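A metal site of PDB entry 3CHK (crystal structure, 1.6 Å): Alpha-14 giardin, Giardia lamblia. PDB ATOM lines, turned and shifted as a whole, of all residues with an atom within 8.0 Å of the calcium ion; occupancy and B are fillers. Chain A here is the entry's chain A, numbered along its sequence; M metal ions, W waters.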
ATOM      1  N   ARG A  91     -22.806 -19.577   8.648  1.00  0.00           N
ATOM      2  CA  ARG A  91     -22.168 -20.908   8.522  1.00  0.00           C
ATOM      3  C   ARG A  91     -22.324 -21.562   7.157  1.00  0.00           C
ATOM      4  O   ARG A  91     -21.338 -22.030   6.559  1.00  0.00           O
ATOM      5  CB  ARG A  91     -22.740 -21.860   9.575  1.00  0.00           C
ATOM      6  CG  ARG A  91     -22.207 -23.309   9.465  1.00  0.00           C
ATOM      7  CD  ARG A  91     -20.752 -23.432   9.943  1.00  0.00           C
ATOM      8  NE  ARG A  91     -20.410 -24.854  10.087  1.00  0.00           N
ATOM      9  CZ  ARG A  91     -19.345 -25.345  10.735  1.00  0.00           C
ATOM     10  NH1 ARG A  91     -18.484 -24.553  11.341  1.00  0.00           N
ATOM     11  NH2 ARG A  91     -19.173 -26.672  10.786  1.00  0.00           N
ATOM     12  N   GLY A  92     -23.576 -21.610   6.683  1.00  0.00           N
ATOM     13  CA  GLY A  92     -23.937 -22.214   5.423  1.00  0.00           C
ATOM     14  C   GLY A  92     -23.238 -21.526   4.270  1.00  0.00           C
ATOM     15  O   GLY A  92     -22.894 -22.160   3.272  1.00  0.00           O
ATOM     16  N   ALA A  93     -23.003 -20.223   4.439  1.00  0.00           N
ATOM     17  CA  ALA A  93     -22.390 -19.430   3.376  1.00  0.00           C
ATOM     18  C   ALA A  93     -20.864 -19.533   3.308  1.00  0.00           C
ATOM     19  O   ALA A  93     -20.275 -19.097   2.337  1.00  0.00           O
ATOM     20  CB  ALA A  93     -22.818 -17.935   3.498  1.00  0.00           C
ATOM     21  N   THR A  94     -20.223 -20.130   4.319  1.00  0.00           N
ATOM     22  CA  THR A  94     -18.746 -20.062   4.439  1.00  0.00           C
ATOM     23  C   THR A  94     -18.069 -21.434   4.589  1.00  0.00           C
ATOM     24  O   THR A  94     -17.063 -21.712   3.924  1.00  0.00           O
ATOM     25  CB  THR A  94     -18.311 -19.224   5.602  1.00  0.00           C
ATOM     26  OG1 THR A  94     -18.991 -19.645   6.799  1.00  0.00           O
ATOM     27  CG2 THR A  94     -18.574 -17.702   5.335  1.00  0.00           C
ATOM     28  N   LYS A  95     -18.637 -22.296   5.435  1.00  0.00           N
ATOM     29  CA  LYS A  95     -18.042 -23.622   5.677  1.00  0.00           C
ATOM     30  C   LYS A  95     -17.825 -24.389   4.385  1.00  0.00           C
ATOM     31  O   LYS A  95     -18.753 -24.546   3.589  1.00  0.00           O
ATOM     32  CB  LYS A  95     -18.878 -24.438   6.663  1.00  0.00           C
ATOM     33  CG  LYS A  95     -18.216 -25.779   7.075  1.00  0.00           C
ATOM     34  CD  LYS A  95     -17.045 -25.523   8.025  1.00  0.00           C
ATOM     35  CE  LYS A  95     -16.197 -26.794   8.201  1.00  0.00           C
ATOM     36  NZ  LYS A  95     -15.161 -26.573   9.265  1.00  0.00           N
ATOM     37  N   GLY A  96     -16.597 -24.870   4.184  1.00  0.00           N
ATOM     38  CA  GLY A  96     -16.262 -25.659   3.014  1.00  0.00           C
ATOM     39  C   GLY A  96     -15.993 -24.880   1.738  1.00  0.00           C
ATOM     40  O   GLY A  96     -15.860 -23.648   1.760  1.00  0.00           O
ATOM     41  N   ALA A  97     -15.943 -25.606   0.636  1.00  0.00           N
ATOM     42  CA  ALA A  97     -15.626 -25.075  -0.691  1.00  0.00           C
ATOM     43  C   ALA A  97     -16.417 -23.823  -1.037  1.00  0.00           C
ATOM     44  O   ALA A  97     -17.647 -23.815  -1.010  1.00  0.00           O
ATOM     45  CB  ALA A  97     -15.846 -26.152  -1.757  1.00  0.00           C
ATOM     46  N   GLY A  98     -15.686 -22.767  -1.385  1.00  0.00           N
ATOM     47  CA  GLY A  98     -16.263 -21.532  -1.872  1.00  0.00           C
ATOM     48  C   GLY A  98     -16.979 -20.702  -0.815  1.00  0.00           C
ATOM     49  O   GLY A  98     -16.792 -20.902   0.391  1.00  0.00           O
ATOM     50  N   THR A  99     -17.763 -19.740  -1.304  1.00  0.00           N
ATOM     51  CA  THR A  99     -18.456 -18.752  -0.456  1.00  0.00           C
ATOM     52  C   THR A  99     -19.776 -18.361  -1.109  1.00  0.00           C
ATOM     53  O   THR A  99     -19.834 -18.145  -2.323  1.00  0.00           O
ATOM     54  CB  THR A  99     -17.598 -17.441  -0.272  1.00  0.00           C
ATOM     55  OG1 THR A  99     -16.281 -17.769   0.203  1.00  0.00           O
ATOM     56  CG2 THR A  99     -18.243 -16.499   0.754  1.00  0.00           C
ATOM     57  N   ASP A 100     -20.851 -18.297  -0.326  1.00  0.00           N
ATOM     58  CA  ASP A 100     -22.082 -17.647  -0.786  1.00  0.00           C
ATOM     59  C   ASP A 100     -21.996 -16.160  -0.359  1.00  0.00           C
ATOM     60  O   ASP A 100     -22.471 -15.782   0.714  1.00  0.00           O
ATOM     61  CB  ASP A 100     -23.328 -18.303  -0.172  1.00  0.00           C
ATOM     62  CG  ASP A 100     -24.634 -17.820  -0.820  1.00  0.00           C
ATOM     63  OD1 ASP A 100     -24.679 -16.692  -1.354  1.00  0.00           O
ATOM     64  OD2 ASP A 100     -25.640 -18.560  -0.776  1.00  0.00           O
ATOM     65  N   VAL A 134     -14.173 -16.106  10.466  1.00  0.00           N
ATOM     66  CA  VAL A 134     -14.789 -16.922   9.444  1.00  0.00           C
ATOM     67  C   VAL A 134     -15.098 -16.098   8.188  1.00  0.00           C
ATOM     68  O   VAL A 134     -14.792 -16.526   7.080  1.00  0.00           O
ATOM     69  CB  VAL A 134     -16.011 -17.681   9.997  1.00  0.00           C
ATOM     70  CG1 VAL A 134     -16.918 -18.157   8.896  1.00  0.00           C
ATOM     71  CG2 VAL A 134     -15.490 -18.888  10.759  1.00  0.00           C
ATOM     72  N   LYS A 137     -11.696 -14.878   6.607  1.00  0.00           N
ATOM     73  CA  LYS A 137     -11.049 -16.031   5.982  1.00  0.00           C
ATOM     74  C   LYS A 137     -11.673 -16.347   4.631  1.00  0.00           C
ATOM     75  O   LYS A 137     -10.968 -16.558   3.646  1.00  0.00           O
ATOM     76  CB  LYS A 137     -11.086 -17.268   6.893  1.00  0.00           C
ATOM     77  CG  LYS A 137     -10.384 -18.487   6.305  1.00  0.00           C
ATOM     78  CD  LYS A 137     -10.225 -19.606   7.348  1.00  0.00           C
ATOM     79  CE  LYS A 137      -9.244 -20.671   6.849  1.00  0.00           C
ATOM     80  NZ  LYS A 137      -9.911 -21.561   5.842  1.00  0.00           N
ATOM     81  N   ASP A 138     -13.009 -16.349   4.566  1.00  0.00           N
ATOM     82  CA  ASP A 138     -13.699 -16.710   3.336  1.00  0.00           C
ATOM     83  C   ASP A 138     -13.682 -15.632   2.259  1.00  0.00           C
ATOM     84  O   ASP A 138     -13.593 -15.946   1.077  1.00  0.00           O
ATOM     85  CB  ASP A 138     -15.122 -17.224   3.594  1.00  0.00           C
ATOM     86  CG  ASP A 138     -15.288 -18.703   3.209  1.00  0.00           C
ATOM     87  OD1 ASP A 138     -16.173 -19.047   2.402  1.00  0.00           O
ATOM     88  OD2 ASP A 138     -14.484 -19.516   3.701  1.00  0.00           O
ATOM     89  N   CYS A 139     -13.803 -14.375   2.684  1.00  0.00           N
ATOM     90  CA  CYS A 139     -14.052 -13.281   1.747  1.00  0.00           C
ATOM     91  C   CYS A 139     -12.818 -12.433   1.447  1.00  0.00           C
ATOM     92  O   CYS A 139     -12.812 -11.739   0.441  1.00  0.00           O
ATOM     93  CB  CYS A 139     -15.097 -12.337   2.313  1.00  0.00           C
ATOM     94  SG  CYS A 139     -16.650 -13.182   2.536  1.00  0.00           S
HETATM   95 CA    CA M   1     -15.552 -21.370   2.255  1.00  0.00          CA
HETATM   96  O   HOH W   1     -13.983 -20.772   0.588  1.00  0.00           O
HETATM   97  O   HOH W   2     -13.755 -22.478   3.434  1.00  0.00           O
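The side-chain hydroxyl (OG1) of Thr 94 lies within hydrogen-bond range of the backbone carbonyl oxygen (O) of Arg 91 (3.4 Å).
O of Asp 138 sits close to OG1 of Thr 99.
The calcium ion is bound by the backbone carbonyl oxygen (O) of Thr 94 (2.3 Å), the backbone carbonyl oxygen (O) of Gly 98 (2.3 Å), the backbone carbonyl oxygen (O) of Gly 96 (2.4 Å), water W1 (2.4 Å), the side-chain carboxylate (OD1) of Asp 138 (2.4 Å), water W2 (2.4 Å) and the side-chain carboxylate (OD2) of Asp 138 (2.6 Å).
The calcium ion has seven donor atoms within binding distance.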
